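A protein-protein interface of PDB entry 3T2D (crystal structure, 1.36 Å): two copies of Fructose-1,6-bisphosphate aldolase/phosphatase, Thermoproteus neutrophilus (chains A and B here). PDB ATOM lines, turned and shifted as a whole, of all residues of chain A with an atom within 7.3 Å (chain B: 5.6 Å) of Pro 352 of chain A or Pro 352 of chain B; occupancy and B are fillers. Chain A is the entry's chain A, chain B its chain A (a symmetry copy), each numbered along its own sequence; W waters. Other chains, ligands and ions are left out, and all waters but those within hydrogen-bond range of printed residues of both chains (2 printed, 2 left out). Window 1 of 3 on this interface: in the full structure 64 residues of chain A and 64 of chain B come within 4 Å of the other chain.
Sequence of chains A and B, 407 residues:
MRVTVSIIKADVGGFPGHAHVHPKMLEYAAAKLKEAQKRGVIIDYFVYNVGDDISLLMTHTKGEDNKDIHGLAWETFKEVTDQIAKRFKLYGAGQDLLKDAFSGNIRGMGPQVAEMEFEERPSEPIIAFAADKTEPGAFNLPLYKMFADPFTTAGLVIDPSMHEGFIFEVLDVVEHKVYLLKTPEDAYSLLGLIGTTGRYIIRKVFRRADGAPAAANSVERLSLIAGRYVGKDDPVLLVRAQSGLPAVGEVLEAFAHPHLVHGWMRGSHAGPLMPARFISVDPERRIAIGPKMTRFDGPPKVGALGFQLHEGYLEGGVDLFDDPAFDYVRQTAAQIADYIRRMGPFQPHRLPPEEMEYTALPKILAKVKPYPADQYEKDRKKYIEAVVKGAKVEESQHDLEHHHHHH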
ATOM      1  N   GLY A 195     -16.373  23.408  18.883  1.00  0.00           N
ATOM      2  CA  GLY A 195     -14.928  23.306  19.092  1.00  0.00           C
ATOM      3  C   GLY A 195     -14.096  23.770  17.941  1.00  0.00           C
ATOM      4  O   GLY A 195     -12.932  24.126  18.101  1.00  0.00           O
ATOM      5  N   THR A 196     -14.689  23.782  16.728  1.00  0.00           N
ATOM      6  CA  THR A 196     -14.042  24.315  15.514  1.00  0.00           C
ATOM      7  C   THR A 196     -14.363  25.789  15.496  1.00  0.00           C
ATOM      8  O   THR A 196     -15.312  26.279  14.833  1.00  0.00           O
ATOM      9  CB  THR A 196     -14.489  23.596  14.277  1.00  0.00           C
ATOM     10  OG1 THR A 196     -14.267  22.212  14.458  1.00  0.00           O
ATOM     11  CG2 THR A 196     -13.776  24.136  13.036  1.00  0.00           C
ATOM     12  N   ARG A 228      -8.984  33.307  -0.360  1.00  0.00           N
ATOM     13  CA  ARG A 228      -8.895  33.146   1.075  1.00  0.00           C
ATOM     14  C   ARG A 228     -10.269  33.514   1.711  1.00  0.00           C
ATOM     15  O   ARG A 228     -11.015  34.449   1.229  1.00  0.00           O
ATOM     16  CB  ARG A 228      -7.757  34.023   1.715  1.00  0.00           C
ATOM     17  CG  ARG A 228      -6.315  33.708   1.240  1.00  0.00           C
ATOM     18  CD  ARG A 228      -5.239  34.285   2.258  1.00  0.00           C
ATOM     19  NE  ARG A 228      -5.099  33.693   3.610  1.00  0.00           N
ATOM     20  CZ  ARG A 228      -4.595  32.487   3.846  1.00  0.00           C
ATOM     21  NH1 ARG A 228      -4.283  31.681   2.794  1.00  0.00           N
ATOM     22  NH2 ARG A 228      -4.364  32.036   5.089  1.00  0.00           N
ATOM     23  N   HIS A 262      -7.750  32.205  19.031  1.00  0.00           N
ATOM     24  CA  HIS A 262      -7.109  32.533  17.781  1.00  0.00           C
ATOM     25  C   HIS A 262      -7.124  33.982  17.528  1.00  0.00           C
ATOM     26  O   HIS A 262      -8.153  34.654  17.715  1.00  0.00           O
ATOM     27  CB  HIS A 262      -7.831  31.846  16.642  1.00  0.00           C
ATOM     28  CG  HIS A 262      -7.790  30.386  16.625  1.00  0.00           C
ATOM     29  ND1 HIS A 262      -7.109  29.504  17.384  1.00  0.00           N
ATOM     30  CD2 HIS A 262      -8.326  29.676  15.616  1.00  0.00           C
ATOM     31  CE1 HIS A 262      -7.413  28.242  16.955  1.00  0.00           C
ATOM     32  NE2 HIS A 262      -8.043  28.375  15.823  1.00  0.00           N
ATOM     33  N   SER A 268      -2.960  35.697  13.353  1.00  0.00           N
ATOM     34  CA  SER A 268      -2.335  34.460  12.871  1.00  0.00           C
ATOM     35  C   SER A 268      -1.720  33.599  13.961  1.00  0.00           C
ATOM     36  O   SER A 268      -0.977  32.681  13.670  1.00  0.00           O
ATOM     37  CB  SER A 268      -1.265  34.806  11.832  1.00  0.00           C
ATOM     38  OG  SER A 268      -1.831  35.462  10.685  1.00  0.00           O
ATOM     39  N   GLN A 347       3.034  26.066  14.389  1.00  0.00           N
ATOM     40  CA  GLN A 347       1.777  25.599  14.900  1.00  0.00           C
ATOM     41  C   GLN A 347       2.081  24.774  16.152  1.00  0.00           C
ATOM     42  O   GLN A 347       3.086  24.048  16.181  1.00  0.00           O
ATOM     43  CB  GLN A 347       1.077  24.651  13.930  1.00  0.00           C
ATOM     44  CG  GLN A 347       0.383  25.304  12.730  1.00  0.00           C
ATOM     45  CD  GLN A 347      -0.467  24.354  11.948  1.00  0.00           C
ATOM     46  OE1 GLN A 347       0.003  23.953  10.934  1.00  0.00           O
ATOM     47  NE2 GLN A 347      -1.659  23.895  12.396  1.00  0.00           N
ATOM     48  N   PRO A 348       1.178  24.793  17.157  1.00  0.00           N
ATOM     49  CA  PRO A 348      -0.129  25.454  17.165  1.00  0.00           C
ATOM     50  C   PRO A 348      -0.099  26.870  17.716  1.00  0.00           C
ATOM     51  O   PRO A 348      -1.174  27.507  17.825  1.00  0.00           O
ATOM     52  CB  PRO A 348      -0.971  24.572  18.073  1.00  0.00           C
ATOM     53  CG  PRO A 348       0.066  24.022  19.023  1.00  0.00           C
ATOM     54  CD  PRO A 348       1.286  23.792  18.236  1.00  0.00           C
ATOM     55  N   HIS A 349       1.083  27.458  18.026  1.00  0.00           N
ATOM     56  CA  HIS A 349       1.103  28.885  18.325  1.00  0.00           C
ATOM     57  C   HIS A 349       0.782  29.710  17.107  1.00  0.00           C
ATOM     58  O   HIS A 349      -0.019  30.649  17.183  1.00  0.00           O
ATOM     59  CB  HIS A 349       2.448  29.290  18.949  1.00  0.00           C
ATOM     60  CG  HIS A 349       2.547  30.766  19.230  1.00  0.00           C
ATOM     61  ND1 HIS A 349       1.550  31.517  19.853  1.00  0.00           N
ATOM     62  CD2 HIS A 349       3.522  31.654  18.988  1.00  0.00           C
ATOM     63  CE1 HIS A 349       1.971  32.770  19.940  1.00  0.00           C
ATOM     64  NE2 HIS A 349       3.191  32.910  19.415  1.00  0.00           N
ATOM     65  N   ARG A 350       1.402  29.426  15.986  1.00  0.00           N
ATOM     66  CA  ARG A 350       0.937  29.972  14.716  1.00  0.00           C
ATOM     67  C   ARG A 350      -0.297  29.160  14.322  1.00  0.00           C
ATOM     68  O   ARG A 350      -0.380  27.962  14.565  1.00  0.00           O
ATOM     69  CB  ARG A 350       2.031  29.821  13.683  1.00  0.00           C
ATOM     70  CG  ARG A 350       1.867  30.671  12.459  1.00  0.00           C
ATOM     71  CD  ARG A 350       2.300  29.977  11.203  1.00  0.00           C
ATOM     72  NE  ARG A 350       1.400  28.937  10.856  1.00  0.00           N
ATOM     73  CZ  ARG A 350       1.596  27.988   9.917  1.00  0.00           C
ATOM     74  NH1 ARG A 350       0.604  27.175   9.625  1.00  0.00           N
ATOM     75  NH2 ARG A 350       2.766  27.896   9.275  1.00  0.00           N
ATOM     76  N   LEU A 351      -1.272  29.824  13.656  1.00  0.00           N
ATOM     77  CA  LEU A 351      -2.493  29.152  13.302  1.00  0.00           C
ATOM     78  C   LEU A 351      -2.367  28.236  12.078  1.00  0.00           C
ATOM     79  O   LEU A 351      -1.398  28.328  11.326  1.00  0.00           O
ATOM     80  CB  LEU A 351      -3.542  30.206  13.026  1.00  0.00           C
ATOM     81  CG  LEU A 351      -4.035  30.992  14.279  1.00  0.00           C
ATOM     82  CD1 LEU A 351      -5.129  31.999  13.808  1.00  0.00           C
ATOM     83  CD2 LEU A 351      -4.435  30.142  15.426  1.00  0.00           C
ATOM     84  N   PRO A 352      -3.355  27.361  11.902  1.00  0.00           N
ATOM     85  CA  PRO A 352      -3.367  26.532  10.706  1.00  0.00           C
ATOM     86  C   PRO A 352      -3.387  27.397   9.478  1.00  0.00           C
ATOM     87  O   PRO A 352      -3.858  28.535   9.486  1.00  0.00           O
ATOM     88  CB  PRO A 352      -4.682  25.714  10.899  1.00  0.00           C
ATOM     89  CG  PRO A 352      -5.007  25.803  12.319  1.00  0.00           C
ATOM     90  CD  PRO A 352      -4.512  27.105  12.773  1.00  0.00           C
ATOM     91  N   PRO A 353      -2.852  26.923   8.374  1.00  0.00           N
ATOM     92  CA  PRO A 353      -2.582  27.791   7.265  1.00  0.00           C
ATOM     93  C   PRO A 353      -3.803  28.522   6.686  1.00  0.00           C
ATOM     94  O   PRO A 353      -3.673  29.696   6.338  1.00  0.00           O
ATOM     95  CB  PRO A 353      -1.929  26.893   6.191  1.00  0.00           C
ATOM     96  CG  PRO A 353      -1.871  25.651   6.709  1.00  0.00           C
ATOM     97  CD  PRO A 353      -2.314  25.593   8.165  1.00  0.00           C
ATOM     98  N   GLU A 354      -4.956  27.850   6.694  1.00  0.00           N
ATOM     99  CA  GLU A 354      -6.180  28.388   6.173  1.00  0.00           C
ATOM    100  C   GLU A 354      -6.796  29.416   7.097  1.00  0.00           C
ATOM    101  O   GLU A 354      -7.611  30.255   6.650  1.00  0.00           O
ATOM    102  CB  GLU A 354      -7.206  27.249   5.951  1.00  0.00           C
ATOM    103  CG  GLU A 354      -7.871  26.458   7.389  1.00  0.00           C
ATOM    104  CD  GLU A 354      -6.941  25.348   8.190  1.00  0.00           C
ATOM    105  OE1 GLU A 354      -5.684  25.210   7.615  1.00  0.00           O
ATOM    106  OE2 GLU A 354      -7.544  24.709   9.376  1.00  0.00           O
ATOM    107  N   GLU A 355      -6.376  29.451   8.362  1.00  0.00           N
ATOM    108  CA  GLU A 355      -6.835  30.346   9.435  1.00  0.00           C
ATOM    109  C   GLU A 355      -6.004  31.564   9.631  1.00  0.00           C
ATOM    110  O   GLU A 355      -6.392  32.505  10.355  1.00  0.00           O
ATOM    111  CB  GLU A 355      -7.106  29.560  10.756  1.00  0.00           C
ATOM    112  CG  GLU A 355      -8.053  28.245  10.556  1.00  0.00           C
ATOM    113  CD  GLU A 355      -8.604  27.371  11.853  1.00  0.00           C
ATOM    114  OE1 GLU A 355      -9.289  28.173  12.617  1.00  0.00           O
ATOM    115  OE2 GLU A 355      -8.472  25.963  12.063  1.00  0.00           O
ATOM    116  N   MET A 356      -4.853  31.655   8.968  1.00  0.00           N
ATOM    117  CA  MET A 356      -3.926  32.805   9.061  1.00  0.00           C
ATOM    118  C   MET A 356      -4.414  34.014   8.292  1.00  0.00           C
ATOM    119  O   MET A 356      -4.722  33.873   7.116  1.00  0.00           O
ATOM    120  CB  MET A 356      -2.576  32.415   8.498  1.00  0.00           C
ATOM    121  CG  MET A 356      -1.939  31.282   9.274  1.00  0.00           C
ATOM    122  SD  MET A 356      -0.219  31.755   9.489  1.00  0.00           S
ATOM    123  CE  MET A 356       0.309  31.277   7.918  1.00  0.00           C
ATOM    124  N   GLU A 357      -4.476  35.169   8.924  1.00  0.00           N
ATOM    125  CA  GLU A 357      -4.828  36.376   8.236  1.00  0.00           C
ATOM    126  C   GLU A 357      -3.715  36.874   7.348  1.00  0.00           C
ATOM    127  O   GLU A 357      -3.960  37.560   6.316  1.00  0.00           O
ATOM    128  CB  GLU A 357      -5.248  37.436   9.279  1.00  0.00           C
ATOM    129  CG  GLU A 357      -5.643  38.806   8.748  1.00  0.00           C
ATOM    130  CD  GLU A 357      -6.134  39.755   9.803  1.00  0.00           C
ATOM    131  OE1 GLU A 357      -6.227  39.359  10.976  1.00  0.00           O
ATOM    132  OE2 GLU A 357      -6.518  40.901   9.487  1.00  0.00           O
ATOM    133  N   HIS B 262       1.219  18.417  18.202  1.00  0.00           N
ATOM    134  CA  HIS B 262      -0.031  17.789  17.851  1.00  0.00           C
ATOM    135  C   HIS B 262      -0.008  16.344  18.126  1.00  0.00           C
ATOM    136  O   HIS B 262       0.970  15.647  17.805  1.00  0.00           O
ATOM    137  CB  HIS B 262      -0.305  17.986  16.375  1.00  0.00           C
ATOM    138  CG  HIS B 262      -0.523  19.359  15.926  1.00  0.00           C
ATOM    139  ND1 HIS B 262      -0.653  20.512  16.612  1.00  0.00           N
ATOM    140  CD2 HIS B 262      -0.855  19.642  14.654  1.00  0.00           C
ATOM    141  CE1 HIS B 262      -0.853  21.525  15.718  1.00  0.00           C
ATOM    142  NE2 HIS B 262      -1.092  20.965  14.567  1.00  0.00           N
ATOM    143  N   GLN B 347     -10.655  24.020  19.981  1.00  0.00           N
ATOM    144  CA  GLN B 347      -9.433  24.469  19.377  1.00  0.00           C
ATOM    145  C   GLN B 347      -8.955  25.679  20.182  1.00  0.00           C
ATOM    146  O   GLN B 347      -9.782  26.493  20.620  1.00  0.00           O
ATOM    147  CB  GLN B 347      -9.645  24.968  17.951  1.00  0.00           C
ATOM    148  CG  GLN B 347      -9.817  23.889  16.876  1.00  0.00           C
ATOM    149  CD  GLN B 347      -9.794  24.431  15.483  1.00  0.00           C
ATOM    150  OE1 GLN B 347     -10.851  24.543  14.954  1.00  0.00           O
ATOM    151  NE2 GLN B 347      -8.661  24.861  14.880  1.00  0.00           N
ATOM    152  N   ARG B 350      -7.987  21.170  21.106  1.00  0.00           N
ATOM    153  CA  ARG B 350      -8.390  20.196  20.097  1.00  0.00           C
ATOM    154  C   ARG B 350      -7.810  20.686  18.769  1.00  0.00           C
ATOM    155  O   ARG B 350      -7.736  21.880  18.504  1.00  0.00           O
ATOM    156  CB  ARG B 350      -9.899  20.142  20.037  1.00  0.00           C
ATOM    157  CG  ARG B 350     -10.463  18.935  19.350  1.00  0.00           C
ATOM    158  CD  ARG B 350     -11.683  19.240  18.535  1.00  0.00           C
ATOM    159  NE  ARG B 350     -11.354  19.999  17.384  1.00  0.00           N
ATOM    160  CZ  ARG B 350     -12.222  20.618  16.556  1.00  0.00           C
ATOM    161  NH1 ARG B 350     -11.759  21.170  15.455  1.00  0.00           N
ATOM    162  NH2 ARG B 350     -13.530  20.642  16.836  1.00  0.00           N
ATOM    163  N   LEU B 351      -7.424  19.732  17.888  1.00  0.00           N
ATOM    164  CA  LEU B 351      -6.813  20.104  16.641  1.00  0.00           C
ATOM    165  C   LEU B 351      -7.807  20.593  15.581  1.00  0.00           C
ATOM    166  O   LEU B 351      -9.012  20.384  15.712  1.00  0.00           O
ATOM    167  CB  LEU B 351      -6.071  18.898  16.108  1.00  0.00           C
ATOM    168  CG  LEU B 351      -4.796  18.498  16.910  1.00  0.00           C
ATOM    169  CD1 LEU B 351      -4.152  17.269  16.197  1.00  0.00           C
ATOM    170  CD2 LEU B 351      -3.858  19.613  17.179  1.00  0.00           C
ATOM    171  N   PRO B 352      -7.281  21.240  14.543  1.00  0.00           N
ATOM    172  CA  PRO B 352      -8.144  21.638  13.440  1.00  0.00           C
ATOM    173  C   PRO B 352      -8.817  20.432  12.849  1.00  0.00           C
ATOM    174  O   PRO B 352      -8.318  19.307  12.912  1.00  0.00           O
ATOM    175  CB  PRO B 352      -7.126  22.310  12.467  1.00  0.00           C
ATOM    176  CG  PRO B 352      -5.954  22.638  13.272  1.00  0.00           C
ATOM    177  CD  PRO B 352      -5.878  21.617  14.321  1.00  0.00           C
ATOM    178  N   PRO B 353      -9.989  20.592  12.276  1.00  0.00           N
ATOM    179  CA  PRO B 353     -10.803  19.456  11.956  1.00  0.00           C
ATOM    180  C   PRO B 353     -10.167  18.437  10.997  1.00  0.00           C
ATOM    181  O   PRO B 353     -10.348  17.238  11.213  1.00  0.00           O
ATOM    182  CB  PRO B 353     -12.097  20.039  11.345  1.00  0.00           C
ATOM    183  CG  PRO B 353     -11.957  21.378  11.348  1.00  0.00           C
ATOM    184  CD  PRO B 353     -10.691  21.841  12.056  1.00  0.00           C
ATOM    185  N   GLU B 354      -9.373  18.932  10.045  1.00  0.00           N
ATOM    186  CA  GLU B 354      -8.721  18.113   9.065  1.00  0.00           C
ATOM    187  C   GLU B 354      -7.535  17.365   9.636  1.00  0.00           C
ATOM    188  O   GLU B 354      -7.107  16.336   9.067  1.00  0.00           O
ATOM    189  CB  GLU B 354      -8.227  18.989   7.888  1.00  0.00           C
ATOM    190  CG  GLU B 354      -6.894  20.109   8.207  1.00  0.00           C
ATOM    191  CD  GLU B 354      -7.213  21.520   9.011  1.00  0.00           C
ATOM    192  OE1 GLU B 354      -8.549  21.620   9.378  1.00  0.00           O
ATOM    193  OE2 GLU B 354      -6.070  22.425   9.243  1.00  0.00           O
ATOM    194  N   GLU B 355      -7.032  17.784  10.798  1.00  0.00           N
ATOM    195  CA  GLU B 355      -5.886  17.228  11.532  1.00  0.00           C
ATOM    196  C   GLU B 355      -6.239  16.245  12.591  1.00  0.00           C
ATOM    197  O   GLU B 355      -5.366  15.543  13.143  1.00  0.00           O
ATOM    198  CB  GLU B 355      -4.924  18.354  12.026  1.00  0.00           C
ATOM    199  CG  GLU B 355      -4.498  19.412  10.858  1.00  0.00           C
ATOM    200  CD  GLU B 355      -3.351  20.581  11.127  1.00  0.00           C
ATOM    201  OE1 GLU B 355      -2.244  19.986  11.470  1.00  0.00           O
ATOM    202  OE2 GLU B 355      -3.486  21.987  10.911  1.00  0.00           O
ATOM    203  N   MET B 356      -7.524  16.088  12.901  1.00  0.00           N
ATOM    204  CA  MET B 356      -8.025  15.149  13.929  1.00  0.00           C
ATOM    205  C   MET B 356      -8.006  13.708  13.464  1.00  0.00           C
ATOM    206  O   MET B 356      -8.549  13.430  12.403  1.00  0.00           O
ATOM    207  CB  MET B 356      -9.454  15.499  14.285  1.00  0.00           C
ATOM    208  CG  MET B 356      -9.571  16.888  14.875  1.00  0.00           C
ATOM    209  SD  MET B 356     -10.672  16.720  16.285  1.00  0.00           S
ATOM    210  CE  MET B 356     -12.143  16.734  15.381  1.00  0.00           C
HETATM  211  O   HOH W   1      -0.345  21.358  10.225  1.00  0.00           O
HETATM  212  O   HOH W   2     -11.360  26.717  13.412  1.00  0.00           O
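Gln 347 of chain A touches Glu 355 of chain B, and with the chains exchanged Glu 355 of chain A touches Gln 347 of chain B.
Pro 352 of chain A touches Glu 354 of chain B, and with the chains exchanged Glu 354 of chain A touches Pro 352 of chain B.
Pro 352 of chain A touches Glu 355 of chain B, and with the chains exchanged Glu 355 of chain A touches Pro 352 of chain B.
Glu 354 of chain A touches its own counterpart, Glu 354 of chain B.
Of the 16 pairs that touch across the chains among the printed residues, 10 have their exchanged pair printed and touching as well.
A ring nitrogen (NE2) of His 262 of chain B lies within hydrogen-bond range of the side-chain carboxylate (OE1) of Glu 355 of chain B, 3.4 Å away.
The side-chain sulfur of Met 356 of chain B sits at hydrogen-bond distance from the guanidinium group of Arg 350 of chain B, at 3.5 Å.
A ring nitrogen (NE2) of His 262 of chain A lies within hydrogen-bond range of the side-chain carboxylate of Glu 355 of chain A.
Hydrophobic or aromatic side chains of chain B that line the printed part of chain A: His 262, Pro 352 and Pro 353.
Pro 352 of chain A touches just these residues of chain B: Pro 352 (3.4 Å), Glu 354 (3.9 Å) and Glu 355 (3.9 Å).
Pro 352 of chain B touches just these residues of chain A: Pro 352, Glu 354 and Glu 355.
Of the printed residues of chain A, His 262 of chain B touches Gln 347 and Pro 348.
Printed residues of chain B within 4 Å of Pro 348 of chain A: His 262.
Printed residues of chain B within 4 Å of Gly 195 of chain A: Gln 347 and Arg 350.
Of the printed residues of chain A, Arg 350 of chain B touches Gly 195 (3.4 Å) and Thr 196 (2.9 Å).
Printed residues of chain B within 4 Å of Glu 355 of chain A: Gln 347 (3.0 Å) and Pro 352 (3.9 Å).
The nearest residue of chain B that does not touch Pro 352 of chain A is Gln 347 of chain B (4.6 Å).
The nearest residue of chain A that does not touch Pro 352 of chain B is Gln 347 of chain A (4.6 Å).
The nearest printed residue of chain B that does not touch His 262 of chain A is Arg 350 of chain B (6.6 Å).
NH2 of Arg 350 of chain B touches C of Gly 195 of chain A (3.4 Å).
Gln 347 of chain B touches Thr 196 of chain A (OE1 to CA, 3.2 Å).
CG2 of Thr 196 of chain A touches CG of Pro 353 of chain B, 3.7 Å away.
Gln 347 of chain B touches His 262 of chain A (NE2 to NE2, 3.7 Å).
NE2 of Gln 347 of chain A touches NE2 of His 262 of chain B, 3.7 Å away.
CB of Pro 348 of chain A touches CE1 of His 262 of chain B, 3.9 Å away.
Pro 352 of chain A touches Pro 352 of chain B (CG to CG, 3.4 Å).
Pro 352 of chain A touches Glu 354 of chain B.
CB of Pro 352 of chain A touches OE2 of Glu 355 of chain B, 3.9 Å away.
CB of Pro 352 of chain B touches OE2 of Glu 355 of chain A, at 3.9 Å.
Water W2 lies within hydrogen-bond range of the side-chain carboxylate (OE1) of Glu 355 of chain A (2.7 Å) and the side-chain amide oxygen (OE1) of Gln 347 of chain B (2.7 Å).
Water W1 lies within hydrogen-bond range of the side-chain carboxylate of Glu 355 of chain B and the side-chain amide oxygen of Gln 347 of chain A.
The side-chain carboxylate (OE2) of Glu 354 of chain A lies close to the side-chain carboxylate (OE2) of Glu 354 of chain B, at 2.7 Å.
The side-chain hydroxyl (OG1) of Thr 196 of chain A sits at hydrogen-bond distance from the guanidinium group (NH1) of Arg 350 of chain B, 2.9 Å away.
NE2 of Gln 347 of chain B lies within hydrogen-bond range of OE2 of Glu 355 of chain A, at 3.0 Å.
The backbone NH (N) of Gln 347 of chain B sits at hydrogen-bond distance from the backbone carbonyl oxygen (O) of Gly 195 of chain A (3.0 Å).
The side-chain carboxylate of Glu 355 of chain B sits at hydrogen-bond distance from the side-chain amide nitrogen of Gln 347 of chain A, 3.0 Å away.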
